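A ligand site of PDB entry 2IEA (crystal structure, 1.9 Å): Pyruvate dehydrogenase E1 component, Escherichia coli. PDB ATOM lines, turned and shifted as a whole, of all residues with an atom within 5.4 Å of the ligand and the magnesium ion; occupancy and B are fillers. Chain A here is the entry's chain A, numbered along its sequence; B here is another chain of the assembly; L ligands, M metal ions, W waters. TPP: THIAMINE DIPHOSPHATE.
O of Ile 569 of chain B is in hydrogen-bond range of N of Glu 235 (3.1 Å). The guanidinium group of Arg 606 of chain B lies within hydrogen-bond range of the backbone carbonyl oxygen of Met 194 (2.8 Å). The backbone NH (N) of Asp 230 sits at hydrogen-bond distance from the backbone carbonyl oxygen (O) of Asn 258 (3.3 Å). O of Ser 109 lies within hydrogen-bond range of OG of Ser 112 (2.7 Å). The backbone NH (N) of Glu 571 of chain B sits at hydrogen-bond distance from the side-chain carboxylate (OE2) of Glu 235 (3.5 Å). The guanidinium group of Arg 606 of chain B lies within salt-bridge range of the side-chain carboxylate of Asp 609, at 2.9 Å. The guanidinium group (NH1) of Arg 606 of chain B sits at hydrogen-bond distance from the side-chain hydroxyl (OG) of Ser 193 (3.1 Å). OD2 of Asp 521 of chain B is in hydrogen-bond range of N of Leu 264, at 2.9 Å.
The magnesium ion is bound by the side-chain amide oxygen (OD1) of Asn 260 (2.1 Å), the side-chain carboxylate (OD2) of Asp 230 (2.2 Å), water W4 (2.2 Å), the backbone carbonyl oxygen (O) of Gln 262 (2.3 Å), an oxygen (O2A) of the ligand (2.5 Å) and an oxygen (O3B) of the ligand (2.5 Å). The magnesium ion has six donor atoms within binding distance.
Water W4 lies within hydrogen-bond range of O of Asn 258 (2.5 Å), O2B of the ligand (2.7 Å), N of Asp 230 (3.1 Å) and ND2 of Asn 260 (3.2 Å). Water W1 lies within hydrogen-bond range of an oxygen (O1A) of the ligand (2.8 Å), the side-chain amide nitrogen of Gln 140 (2.8 Å), the side-chain carboxylate of Glu 232 (2.9 Å) and the backbone NH of Gly 229 (3.3 Å). Water W5 bridges NE2 of His 640 of chain B and N4' of the ligand. Water W3 bridges OE2 of Glu 522 of chain B (2.8 Å) and OH of Tyr 599 of chain B (3.4 Å).
A nitrogen (N3) of the ligand sits close to the side-chain carboxylate of Glu 522 of chain B, at 3.1 Å. Ser 193 touches the ligand (CA to N3', 3.8 Å). CA of Gly 229 touches O1A of the ligand (3.5 Å). OE1 of Glu 235 touches CM2 of the ligand, 3.3 Å away. Asn 258 touches the ligand. Arg 263 touches the ligand. Leu 264 touches the ligand (N to C6, 3.5 Å). Lys 392 touches the ligand. OD2 of Asp 521 of chain B touches CM4 of the ligand, 3.3 Å away. Ile 569 of chain B touches the ligand (CD1 to O7, 3.4 Å). CE1 of Phe 602 of chain B touches C2' of the ligand (3.4 Å). Arg 606 of chain B touches the ligand (NH1 to CM2, 3.7 Å). His 640 of chain B touches the ligand (NE2 to N4', 3.9 Å). Within 4 Å of the ligand: Ser 109, Gln 140, His 142, Val 192, Ser 193, Met 194, Gly 229, Asp 230, Gly 231, Glu 232, Glu 235, Asn 258, Asn 260, Gln 262, Arg 263, Leu 264, Lys 392, Asp 521 of chain B, Glu 522 of chain B, Ile 569 of chain B, Glu 571 of chain B, Phe 602 of chain B, Arg 606 of chain B and His 640 of chain B. Along chain A the residues within 4 Å of the ligand span positions 109 to 392.
The backbone NH (N) of Glu 232 is in hydrogen-bond range of an oxygen (O1A) of the ligand, at 3.0 Å. The backbone carbonyl oxygen (O) of Val 192 lies within hydrogen-bond range of a nitrogen (N4') of the ligand (2.8 Å). NE2 of Gln 140 is in hydrogen-bond range of O2B of the ligand (3.3 Å). The backbone NH of Gly 231 lies close to an oxygen (O2A) of the ligand, at 2.8 Å. N1' of the ligand sits at hydrogen-bond distance from OE2 of Glu 571 of chain B (2.8 Å). OG of Ser 109 is in hydrogen-bond range of O2B of the ligand (3.0 Å). The backbone NH (N) of Met 194 sits at hydrogen-bond distance from a nitrogen (N3') of the ligand, 3.2 Å away. An oxygen (O1B) of the ligand is in hydrogen-bond range of a ring nitrogen (NE2) of His 142 (2.6 Å).
Residues that only touch the magnesium ion: Asn 258 (3.9 Å). Four residues have an atom within 4 Å of the magnesium ion: Asp 230, Asn 258, Asn 260 and Gln 262. Along chain A the residues within 4 Å of the magnesium ion span positions 230 to 262. The nearest printed residue that does not touch the magnesium ion is Gly 231 (4.1 Å).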
ATOM      1  N   HIS A 106      16.769 -27.280 -26.886  1.00  0.00           N
ATOM      2  CA  HIS A 106      17.998 -27.548 -26.127  1.00  0.00           C
ATOM      3  C   HIS A 106      17.936 -28.828 -25.298  1.00  0.00           C
ATOM      4  O   HIS A 106      16.846 -29.320 -24.970  1.00  0.00           O
ATOM      5  CB  HIS A 106      18.274 -26.370 -25.191  1.00  0.00           C
ATOM      6  CG  HIS A 106      18.112 -25.035 -25.850  1.00  0.00           C
ATOM      7  ND1 HIS A 106      19.181 -24.283 -26.290  1.00  0.00           N
ATOM      8  CD2 HIS A 106      17.000 -24.318 -26.153  1.00  0.00           C
ATOM      9  CE1 HIS A 106      18.749 -23.167 -26.835  1.00  0.00           C
ATOM     10  NE2 HIS A 106      17.428 -23.161 -26.773  1.00  0.00           N
ATOM     11  N   SER A 109      21.178 -27.922 -21.036  1.00  0.00           N
ATOM     12  CA  SER A 109      20.756 -27.224 -19.822  1.00  0.00           C
ATOM     13  C   SER A 109      19.882 -28.078 -18.912  1.00  0.00           C
ATOM     14  O   SER A 109      20.157 -28.179 -17.723  1.00  0.00           O
ATOM     15  CB  SER A 109      20.015 -25.943 -20.183  1.00  0.00           C
ATOM     16  OG  SER A 109      19.760 -25.188 -19.007  1.00  0.00           O
ATOM     17  N   SER A 112      21.663 -30.588 -16.901  1.00  0.00           N
ATOM     18  CA  SER A 112      22.398 -30.087 -15.743  1.00  0.00           C
ATOM     19  C   SER A 112      21.520 -29.739 -14.546  1.00  0.00           C
ATOM     20  O   SER A 112      21.982 -29.763 -13.421  1.00  0.00           O
ATOM     21  CB  SER A 112      23.251 -28.860 -16.137  1.00  0.00           C
ATOM     22  OG  SER A 112      22.464 -27.698 -16.331  1.00  0.00           O
ATOM     23  N   GLN A 140      12.866 -22.213 -15.836  1.00  0.00           N
ATOM     24  CA  GLN A 140      13.822 -21.623 -16.772  1.00  0.00           C
ATOM     25  C   GLN A 140      13.320 -22.023 -18.170  1.00  0.00           C
ATOM     26  O   GLN A 140      13.092 -23.202 -18.445  1.00  0.00           O
ATOM     27  CB  GLN A 140      15.213 -22.208 -16.509  1.00  0.00           C
ATOM     28  CG  GLN A 140      16.304 -21.703 -17.437  1.00  0.00           C
ATOM     29  CD  GLN A 140      17.637 -22.327 -17.098  1.00  0.00           C
ATOM     30  OE1 GLN A 140      17.689 -23.499 -16.705  1.00  0.00           O
ATOM     31  NE2 GLN A 140      18.720 -21.571 -17.245  1.00  0.00           N
ATOM     32  N   HIS A 142      14.363 -22.549 -21.450  1.00  0.00           N
ATOM     33  CA  HIS A 142      14.845 -23.618 -22.319  1.00  0.00           C
ATOM     34  C   HIS A 142      14.970 -25.014 -21.739  1.00  0.00           C
ATOM     35  O   HIS A 142      15.537 -25.886 -22.392  1.00  0.00           O
ATOM     36  CB  HIS A 142      16.153 -23.208 -22.996  1.00  0.00           C
ATOM     37  CG  HIS A 142      17.225 -22.791 -22.047  1.00  0.00           C
ATOM     38  ND1 HIS A 142      17.134 -21.644 -21.284  1.00  0.00           N
ATOM     39  CD2 HIS A 142      18.429 -23.334 -21.766  1.00  0.00           C
ATOM     40  CE1 HIS A 142      18.237 -21.509 -20.565  1.00  0.00           C
ATOM     41  NE2 HIS A 142      19.037 -22.519 -20.842  1.00  0.00           N
ATOM     42  N   VAL A 192      11.636 -17.117 -21.024  1.00  0.00           N
ATOM     43  CA  VAL A 192      12.739 -17.171 -21.983  1.00  0.00           C
ATOM     44  C   VAL A 192      13.485 -15.889 -22.241  1.00  0.00           C
ATOM     45  O   VAL A 192      14.657 -15.940 -22.586  1.00  0.00           O
ATOM     46  CB  VAL A 192      12.361 -17.679 -23.375  1.00  0.00           C
ATOM     47  CG1 VAL A 192      12.834 -19.087 -23.510  1.00  0.00           C
ATOM     48  CG2 VAL A 192      10.891 -17.512 -23.647  1.00  0.00           C
ATOM     49  N   SER A 193      12.819 -14.748 -22.131  1.00  0.00           N
ATOM     50  CA  SER A 193      13.558 -13.510 -22.310  1.00  0.00           C
ATOM     51  C   SER A 193      14.239 -13.381 -20.961  1.00  0.00           C
ATOM     52  O   SER A 193      13.632 -12.946 -19.981  1.00  0.00           O
ATOM     53  CB  SER A 193      12.624 -12.327 -22.537  1.00  0.00           C
ATOM     54  OG  SER A 193      13.391 -11.160 -22.748  1.00  0.00           O
ATOM     55  N   MET A 194      15.495 -13.789 -20.907  1.00  0.00           N
ATOM     56  CA  MET A 194      16.236 -13.766 -19.674  1.00  0.00           C
ATOM     57  C   MET A 194      16.280 -12.429 -18.949  1.00  0.00           C
ATOM     58  O   MET A 194      16.303 -11.371 -19.580  1.00  0.00           O
ATOM     59  CB  MET A 194      17.632 -14.303 -19.931  1.00  0.00           C
ATOM     60  CG  MET A 194      17.573 -15.784 -20.285  1.00  0.00           C
ATOM     61  SD  MET A 194      19.089 -16.442 -20.930  1.00  0.00           S
ATOM     62  CE  MET A 194      18.513 -18.069 -21.442  1.00  0.00           C
ATOM     63  N   GLY A 229      19.587 -19.036 -14.685  1.00  0.00           N
ATOM     64  CA  GLY A 229      20.873 -19.538 -15.145  1.00  0.00           C
ATOM     65  C   GLY A 229      21.902 -18.575 -14.591  1.00  0.00           C
ATOM     66  O   GLY A 229      21.556 -17.420 -14.314  1.00  0.00           O
ATOM     67  N   ASP A 230      23.153 -19.011 -14.413  1.00  0.00           N
ATOM     68  CA  ASP A 230      24.146 -18.080 -13.875  1.00  0.00           C
ATOM     69  C   ASP A 230      24.523 -17.014 -14.895  1.00  0.00           C
ATOM     70  O   ASP A 230      24.755 -15.857 -14.539  1.00  0.00           O
ATOM     71  CB  ASP A 230      25.389 -18.831 -13.324  1.00  0.00           C
ATOM     72  CG  ASP A 230      25.947 -19.865 -14.283  1.00  0.00           C
ATOM     73  OD1 ASP A 230      26.845 -20.635 -13.876  1.00  0.00           O
ATOM     74  OD2 ASP A 230      25.512 -19.912 -15.441  1.00  0.00           O
ATOM     75  N   GLY A 231      24.573 -17.387 -16.174  1.00  0.00           N
ATOM     76  CA  GLY A 231      24.878 -16.412 -17.207  1.00  0.00           C
ATOM     77  C   GLY A 231      23.797 -15.342 -17.266  1.00  0.00           C
ATOM     78  O   GLY A 231      24.092 -14.158 -17.461  1.00  0.00           O
ATOM     79  N   GLU A 232      22.548 -15.765 -17.081  1.00  0.00           N
ATOM     80  CA  GLU A 232      21.402 -14.864 -17.095  1.00  0.00           C
ATOM     81  C   GLU A 232      21.478 -13.800 -16.011  1.00  0.00           C
ATOM     82  O   GLU A 232      20.909 -12.705 -16.147  1.00  0.00           O
ATOM     83  CB  GLU A 232      20.101 -15.680 -16.943  1.00  0.00           C
ATOM     84  CG  GLU A 232      18.915 -14.900 -16.371  1.00  0.00           C
ATOM     85  CD  GLU A 232      17.621 -15.700 -16.407  1.00  0.00           C
ATOM     86  OE1 GLU A 232      17.658 -16.927 -16.186  1.00  0.00           O
ATOM     87  OE2 GLU A 232      16.556 -15.087 -16.648  1.00  0.00           O
ATOM     88  N   GLU A 235      22.111 -10.078 -16.799  1.00  0.00           N
ATOM     89  CA  GLU A 235      21.095  -9.117 -17.244  1.00  0.00           C
ATOM     90  C   GLU A 235      20.872  -8.178 -16.067  1.00  0.00           C
ATOM     91  O   GLU A 235      20.714  -8.629 -14.932  1.00  0.00           O
ATOM     92  CB  GLU A 235      19.774  -9.838 -17.581  1.00  0.00           C
ATOM     93  CG  GLU A 235      19.826 -10.755 -18.800  1.00  0.00           C
ATOM     94  CD  GLU A 235      19.852 -10.015 -20.136  1.00  0.00           C
ATOM     95  OE1 GLU A 235      19.597 -10.650 -21.170  1.00  0.00           O
ATOM     96  OE2 GLU A 235      20.133  -8.793 -20.143  1.00  0.00           O
ATOM     97  N   ASN A 258      21.118 -21.956 -11.343  1.00  0.00           N
ATOM     98  CA  ASN A 258      21.833 -23.132 -11.817  1.00  0.00           C
ATOM     99  C   ASN A 258      23.251 -22.693 -12.171  1.00  0.00           C
ATOM    100  O   ASN A 258      23.492 -22.130 -13.246  1.00  0.00           O
ATOM    101  CB  ASN A 258      21.139 -23.732 -13.037  1.00  0.00           C
ATOM    102  CG  ASN A 258      21.831 -24.973 -13.548  1.00  0.00           C
ATOM    103  OD1 ASN A 258      22.798 -25.434 -12.940  1.00  0.00           O
ATOM    104  ND2 ASN A 258      21.346 -25.517 -14.648  1.00  0.00           N
ATOM    105  N   CYS A 259      24.175 -22.945 -11.258  1.00  0.00           N
ATOM    106  CA  CYS A 259      25.558 -22.548 -11.482  1.00  0.00           C
ATOM    107  C   CYS A 259      26.406 -23.613 -12.159  1.00  0.00           C
ATOM    108  O   CYS A 259      27.165 -24.326 -11.507  1.00  0.00           O
ATOM    109  CB  CYS A 259      26.194 -22.136 -10.159  1.00  0.00           C
ATOM    110  SG  CYS A 259      25.368 -20.713  -9.388  1.00  0.00           S
ATOM    111  N   ASN A 260      26.249 -23.745 -13.486  1.00  0.00           N
ATOM    112  CA  ASN A 260      27.050 -24.705 -14.224  1.00  0.00           C
ATOM    113  C   ASN A 260      28.300 -23.986 -14.723  1.00  0.00           C
ATOM    114  O   ASN A 260      29.102 -24.545 -15.479  1.00  0.00           O
ATOM    115  CB  ASN A 260      26.255 -25.328 -15.379  1.00  0.00           C
ATOM    116  CG  ASN A 260      25.484 -24.312 -16.176  1.00  0.00           C
ATOM    117  OD1 ASN A 260      25.947 -23.202 -16.383  1.00  0.00           O
ATOM    118  ND2 ASN A 260      24.298 -24.687 -16.633  1.00  0.00           N
ATOM    119  N   LEU A 261      28.443 -22.740 -14.283  1.00  0.00           N
ATOM    120  CA  LEU A 261      29.595 -21.893 -14.615  1.00  0.00           C
ATOM    121  C   LEU A 261      29.695 -21.424 -16.061  1.00  0.00           C
ATOM    122  O   LEU A 261      30.630 -20.706 -16.415  1.00  0.00           O
ATOM    123  CB  LEU A 261      30.892 -22.615 -14.238  1.00  0.00           C
ATOM    124  CG  LEU A 261      30.991 -23.278 -12.868  1.00  0.00           C
ATOM    125  CD1 LEU A 261      32.328 -23.992 -12.735  1.00  0.00           C
ATOM    126  CD2 LEU A 261      30.833 -22.255 -11.763  1.00  0.00           C
ATOM    127  N   GLN A 262      28.727 -21.808 -16.894  1.00  0.00           N
ATOM    128  CA  GLN A 262      28.792 -21.436 -18.302  1.00  0.00           C
ATOM    129  C   GLN A 262      27.535 -20.783 -18.851  1.00  0.00           C
ATOM    130  O   GLN A 262      26.437 -21.054 -18.413  1.00  0.00           O
ATOM    131  CB  GLN A 262      29.056 -22.693 -19.146  1.00  0.00           C
ATOM    132  CG  GLN A 262      30.068 -23.652 -18.559  1.00  0.00           C
ATOM    133  CD  GLN A 262      30.003 -25.037 -19.194  1.00  0.00           C
ATOM    134  OE1 GLN A 262      30.697 -25.955 -18.764  1.00  0.00           O
ATOM    135  NE2 GLN A 262      29.179 -25.171 -20.229  1.00  0.00           N
ATOM    136  N   ARG A 263      27.721 -19.894 -19.832  1.00  0.00           N
ATOM    137  CA  ARG A 263      26.566 -19.286 -20.476  1.00  0.00           C
ATOM    138  C   ARG A 263      26.491 -20.051 -21.791  1.00  0.00           C
ATOM    139  O   ARG A 263      26.854 -21.220 -21.833  1.00  0.00           O
ATOM    140  CB  ARG A 263      26.764 -17.776 -20.690  1.00  0.00           C
ATOM    141  CG  ARG A 263      28.160 -17.315 -21.017  1.00  0.00           C
ATOM    142  CD  ARG A 263      28.176 -15.791 -21.124  1.00  0.00           C
ATOM    143  NE  ARG A 263      29.529 -15.277 -21.322  1.00  0.00           N
ATOM    144  CZ  ARG A 263      30.270 -15.515 -22.394  1.00  0.00           C
ATOM    145  NH1 ARG A 263      31.494 -15.016 -22.485  1.00  0.00           N
ATOM    146  NH2 ARG A 263      29.785 -16.246 -23.384  1.00  0.00           N
ATOM    147  N   LEU A 264      26.046 -19.423 -22.872  1.00  0.00           N
ATOM    148  CA  LEU A 264      25.949 -20.157 -24.131  1.00  0.00           C
ATOM    149  C   LEU A 264      27.292 -20.394 -24.813  1.00  0.00           C
ATOM    150  O   LEU A 264      27.697 -21.552 -24.992  1.00  0.00           O
ATOM    151  CB  LEU A 264      24.980 -19.437 -25.087  1.00  0.00           C
ATOM    152  CG  LEU A 264      24.335 -20.251 -26.230  1.00  0.00           C
ATOM    153  CD1 LEU A 264      25.309 -20.447 -27.368  1.00  0.00           C
ATOM    154  CD2 LEU A 264      23.841 -21.577 -25.693  1.00  0.00           C
ATOM    155  N   VAL A 268      30.763 -17.950 -17.666  1.00  0.00           N
ATOM    156  CA  VAL A 268      30.299 -16.631 -17.281  1.00  0.00           C
ATOM    157  C   VAL A 268      31.502 -15.751 -16.955  1.00  0.00           C
ATOM    158  O   VAL A 268      31.609 -14.624 -17.436  1.00  0.00           O
ATOM    159  CB  VAL A 268      29.369 -16.706 -16.051  1.00  0.00           C
ATOM    160  CG1 VAL A 268      28.710 -15.354 -15.816  1.00  0.00           C
ATOM    161  CG2 VAL A 268      28.317 -17.786 -16.265  1.00  0.00           C
ATOM    162  N   LYS A 392      27.191 -28.662 -16.952  1.00  0.00           N
ATOM    163  CA  LYS A 392      26.374 -28.403 -18.138  1.00  0.00           C
ATOM    164  C   LYS A 392      26.571 -29.538 -19.138  1.00  0.00           C
ATOM    165  O   LYS A 392      27.691 -29.950 -19.413  1.00  0.00           O
ATOM    166  CB  LYS A 392      26.770 -27.055 -18.758  1.00  0.00           C
ATOM    167  CG  LYS A 392      25.816 -26.564 -19.829  1.00  0.00           C
ATOM    168  CD  LYS A 392      26.022 -25.079 -20.104  1.00  0.00           C
ATOM    169  CE  LYS A 392      25.160 -24.606 -21.253  1.00  0.00           C
ATOM    170  NZ  LYS A 392      25.523 -25.329 -22.500  1.00  0.00           N
ATOM    171  N   ASP A 609       9.981  -4.957 -23.167  1.00  0.00           N
ATOM    172  CA  ASP A 609      10.103  -6.406 -23.202  1.00  0.00           C
ATOM    173  C   ASP A 609       9.148  -7.035 -22.185  1.00  0.00           C
ATOM    174  O   ASP A 609       8.631  -8.127 -22.395  1.00  0.00           O
ATOM    175  CB  ASP A 609      11.540  -6.837 -22.921  1.00  0.00           C
ATOM    176  CG  ASP A 609      11.915  -8.141 -23.629  1.00  0.00           C
ATOM    177  OD1 ASP A 609      12.873  -8.791 -23.179  1.00  0.00           O
ATOM    178  OD2 ASP A 609      11.275  -8.489 -24.644  1.00  0.00           O
ATOM    179  N   ALA B 520      26.421 -10.266 -27.317  1.00  0.00           N
ATOM    180  CA  ALA B 520      25.899 -10.539 -25.997  1.00  0.00           C
ATOM    181  C   ALA B 520      25.828 -12.057 -25.835  1.00  0.00           C
ATOM    182  O   ALA B 520      24.780 -12.657 -26.030  1.00  0.00           O
ATOM    183  CB  ALA B 520      24.512  -9.914 -25.839  1.00  0.00           C
ATOM    184  N   ASP B 521      26.965 -12.639 -25.489  1.00  0.00           N
ATOM    185  CA  ASP B 521      27.124 -14.085 -25.315  1.00  0.00           C
ATOM    186  C   ASP B 521      27.138 -14.804 -26.658  1.00  0.00           C
ATOM    187  O   ASP B 521      28.195 -15.216 -27.138  1.00  0.00           O
ATOM    188  CB  ASP B 521      26.008 -14.667 -24.431  1.00  0.00           C
ATOM    189  CG  ASP B 521      26.178 -16.160 -24.193  1.00  0.00           C
ATOM    190  OD1 ASP B 521      27.271 -16.693 -24.492  1.00  0.00           O
ATOM    191  OD2 ASP B 521      25.224 -16.806 -23.712  1.00  0.00           O
ATOM    192  N   GLU B 522      25.955 -14.941 -27.254  1.00  0.00           N
ATOM    193  CA  GLU B 522      25.795 -15.618 -28.544  1.00  0.00           C
ATOM    194  C   GLU B 522      26.636 -15.044 -29.677  1.00  0.00           C
ATOM    195  O   GLU B 522      26.473 -13.888 -30.070  1.00  0.00           O
ATOM    196  CB  GLU B 522      24.328 -15.600 -28.976  1.00  0.00           C
ATOM    197  CG  GLU B 522      23.593 -16.927 -28.874  1.00  0.00           C
ATOM    198  CD  GLU B 522      23.024 -17.189 -27.497  1.00  0.00           C
ATOM    199  OE1 GLU B 522      23.773 -17.009 -26.509  1.00  0.00           O
ATOM    200  OE2 GLU B 522      21.840 -17.563 -27.393  1.00  0.00           O
ATOM    201  N   ILE B 569      25.220 -12.274 -21.401  1.00  0.00           N
ATOM    202  CA  ILE B 569      23.775 -12.155 -21.482  1.00  0.00           C
ATOM    203  C   ILE B 569      23.386 -10.853 -20.810  1.00  0.00           C
ATOM    204  O   ILE B 569      22.888 -10.825 -19.674  1.00  0.00           O
ATOM    205  CB  ILE B 569      23.095 -13.350 -20.781  1.00  0.00           C
ATOM    206  CG1 ILE B 569      23.738 -14.660 -21.270  1.00  0.00           C
ATOM    207  CG2 ILE B 569      21.604 -13.352 -21.082  1.00  0.00           C
ATOM    208  CD1 ILE B 569      23.167 -15.921 -20.641  1.00  0.00           C
ATOM    209  N   GLU B 571      22.003  -7.427 -22.752  1.00  0.00           N
ATOM    210  CA  GLU B 571      21.784  -6.551 -23.891  1.00  0.00           C
ATOM    211  C   GLU B 571      21.960  -5.070 -23.571  1.00  0.00           C
ATOM    212  O   GLU B 571      22.482  -4.316 -24.382  1.00  0.00           O
ATOM    213  CB  GLU B 571      20.397  -6.782 -24.502  1.00  0.00           C
ATOM    214  CG  GLU B 571      20.270  -8.050 -25.343  1.00  0.00           C
ATOM    215  CD  GLU B 571      20.109  -9.307 -24.514  1.00  0.00           C
ATOM    216  OE1 GLU B 571      19.861  -9.196 -23.292  1.00  0.00           O
ATOM    217  OE2 GLU B 571      20.216 -10.408 -25.088  1.00  0.00           O
ATOM    218  N   TYR B 599      19.938 -10.779 -30.858  1.00  0.00           N
ATOM    219  CA  TYR B 599      18.620 -11.204 -31.334  1.00  0.00           C
ATOM    220  C   TYR B 599      17.799  -9.928 -31.480  1.00  0.00           C
ATOM    221  O   TYR B 599      17.584  -9.230 -30.495  1.00  0.00           O
ATOM    222  CB  TYR B 599      17.947 -12.132 -30.334  1.00  0.00           C
ATOM    223  CG  TYR B 599      18.490 -13.549 -30.306  1.00  0.00           C
ATOM    224  CD1 TYR B 599      19.690 -13.836 -29.660  1.00  0.00           C
ATOM    225  CD2 TYR B 599      17.781 -14.599 -30.870  1.00  0.00           C
ATOM    226  CE1 TYR B 599      20.169 -15.153 -29.579  1.00  0.00           C
ATOM    227  CE2 TYR B 599      18.231 -15.902 -30.801  1.00  0.00           C
ATOM    228  CZ  TYR B 599      19.433 -16.177 -30.148  1.00  0.00           C
ATOM    229  OH  TYR B 599      19.873 -17.471 -30.061  1.00  0.00           O
ATOM    230  N   PHE B 602      15.433  -8.477 -28.849  1.00  0.00           N
ATOM    231  CA  PHE B 602      15.987  -7.906 -27.623  1.00  0.00           C
ATOM    232  C   PHE B 602      16.724  -6.598 -27.865  1.00  0.00           C
ATOM    233  O   PHE B 602      17.608  -6.227 -27.090  1.00  0.00           O
ATOM    234  CB  PHE B 602      16.911  -8.917 -26.953  1.00  0.00           C
ATOM    235  CG  PHE B 602      16.245 -10.250 -26.698  1.00  0.00           C
ATOM    236  CD1 PHE B 602      16.916 -11.433 -26.997  1.00  0.00           C
ATOM    237  CD2 PHE B 602      14.959 -10.317 -26.204  1.00  0.00           C
ATOM    238  CE1 PHE B 602      16.294 -12.667 -26.815  1.00  0.00           C
ATOM    239  CE2 PHE B 602      14.326 -11.537 -26.012  1.00  0.00           C
ATOM    240  CZ  PHE B 602      14.988 -12.721 -26.322  1.00  0.00           C
ATOM    241  N   ARG B 606      13.753  -4.213 -25.755  1.00  0.00           N
ATOM    242  CA  ARG B 606      14.398  -4.436 -24.461  1.00  0.00           C
ATOM    243  C   ARG B 606      15.270  -3.294 -23.950  1.00  0.00           C
ATOM    244  O   ARG B 606      15.340  -3.070 -22.736  1.00  0.00           O
ATOM    245  CB  ARG B 606      15.221  -5.728 -24.547  1.00  0.00           C
ATOM    246  CG  ARG B 606      15.977  -6.123 -23.273  1.00  0.00           C
ATOM    247  CD  ARG B 606      15.054  -6.314 -22.079  1.00  0.00           C
ATOM    248  NE  ARG B 606      15.781  -6.889 -20.957  1.00  0.00           N
ATOM    249  CZ  ARG B 606      15.843  -8.198 -20.692  1.00  0.00           C
ATOM    250  NH1 ARG B 606      15.203  -9.070 -21.461  1.00  0.00           N
ATOM    251  NH2 ARG B 606      16.591  -8.635 -19.688  1.00  0.00           N
ATOM    252  N   HIS B 640      10.676 -14.457 -29.186  1.00  0.00           N
ATOM    253  CA  HIS B 640      11.864 -14.311 -30.022  1.00  0.00           C
ATOM    254  C   HIS B 640      11.543 -13.836 -31.439  1.00  0.00           C
ATOM    255  O   HIS B 640      12.352 -13.127 -32.057  1.00  0.00           O
ATOM    256  CB  HIS B 640      12.590 -15.656 -30.166  1.00  0.00           C
ATOM    257  CG  HIS B 640      13.309 -16.110 -28.935  1.00  0.00           C
ATOM    258  ND1 HIS B 640      12.656 -16.603 -27.829  1.00  0.00           N
ATOM    259  CD2 HIS B 640      14.629 -16.171 -28.657  1.00  0.00           C
ATOM    260  CE1 HIS B 640      13.550 -16.963 -26.919  1.00  0.00           C
ATOM    261  NE2 HIS B 640      14.749 -16.702 -27.395  1.00  0.00           N
HETATM  262  N1' TPP L   1      18.967 -12.798 -24.396  1.00  0.00           N
HETATM  263  C2' TPP L   1      17.742 -12.911 -23.760  1.00  0.00           C
HETATM  264  CM2 TPP L   1      17.164 -11.676 -23.169  1.00  0.00           C
HETATM  265  N3' TPP L   1      17.078 -14.073 -23.671  1.00  0.00           N
HETATM  266  C4' TPP L   1      17.635 -15.218 -24.252  1.00  0.00           C
HETATM  267  N4' TPP L   1      16.917 -16.324 -24.137  1.00  0.00           N
HETATM  268  C5' TPP L   1      18.931 -15.136 -24.949  1.00  0.00           C
HETATM  269  C6' TPP L   1      19.549 -13.904 -24.980  1.00  0.00           C
HETATM  270  C7' TPP L   1      19.570 -16.295 -25.710  1.00  0.00           C
HETATM  271  N3  TPP L   1      20.054 -17.444 -24.839  1.00  0.00           N
HETATM  272  C2  TPP L   1      19.475 -18.635 -24.822  1.00  0.00           C
HETATM  273  S1  TPP L   1      20.284 -19.744 -23.862  1.00  0.00           S
HETATM  274  C5  TPP L   1      21.476 -18.574 -23.443  1.00  0.00           C
HETATM  275  C4  TPP L   1      21.226 -17.375 -24.048  1.00  0.00           C
HETATM  276  CM4 TPP L   1      22.037 -16.107 -23.947  1.00  0.00           C
HETATM  277  C6  TPP L   1      22.573 -18.894 -22.482  1.00  0.00           C
HETATM  278  C7  TPP L   1      22.023 -19.508 -21.223  1.00  0.00           C
HETATM  279  O7  TPP L   1      22.996 -19.308 -20.173  1.00  0.00           O
HETATM  280  PA  TPP L   1      22.594 -19.410 -18.621  1.00  0.00           P
HETATM  281  O1A TPP L   1      21.631 -18.329 -18.299  1.00  0.00           O
HETATM  282  O2A TPP L   1      23.853 -19.475 -17.849  1.00  0.00           O
HETATM  283  O3A TPP L   1      21.827 -20.826 -18.512  1.00  0.00           O
HETATM  284  PB  TPP L   1      22.193 -22.373 -18.779  1.00  0.00           P
HETATM  285  O1B TPP L   1      21.559 -22.765 -20.067  1.00  0.00           O
HETATM  286  O2B TPP L   1      21.526 -23.182 -17.627  1.00  0.00           O
HETATM  287  O3B TPP L   1      23.661 -22.525 -18.708  1.00  0.00           O
HETATM  288 MG    MG M   1      24.881 -21.451 -16.819  1.00  0.00          MG
HETATM  289  O   HOH W   1      18.924 -18.882 -17.946  1.00  0.00           O
HETATM  290  O   HOH W   2      22.252 -12.492 -24.598  1.00  0.00           O
HETATM  291  O   HOH W   3      20.319 -19.875 -27.764  1.00  0.00           O
HETATM  292  O   HOH W   4      22.978 -21.871 -15.710  1.00  0.00           O
HETATM  293  O   HOH W   5      16.742 -18.507 -26.361  1.00  0.00           O
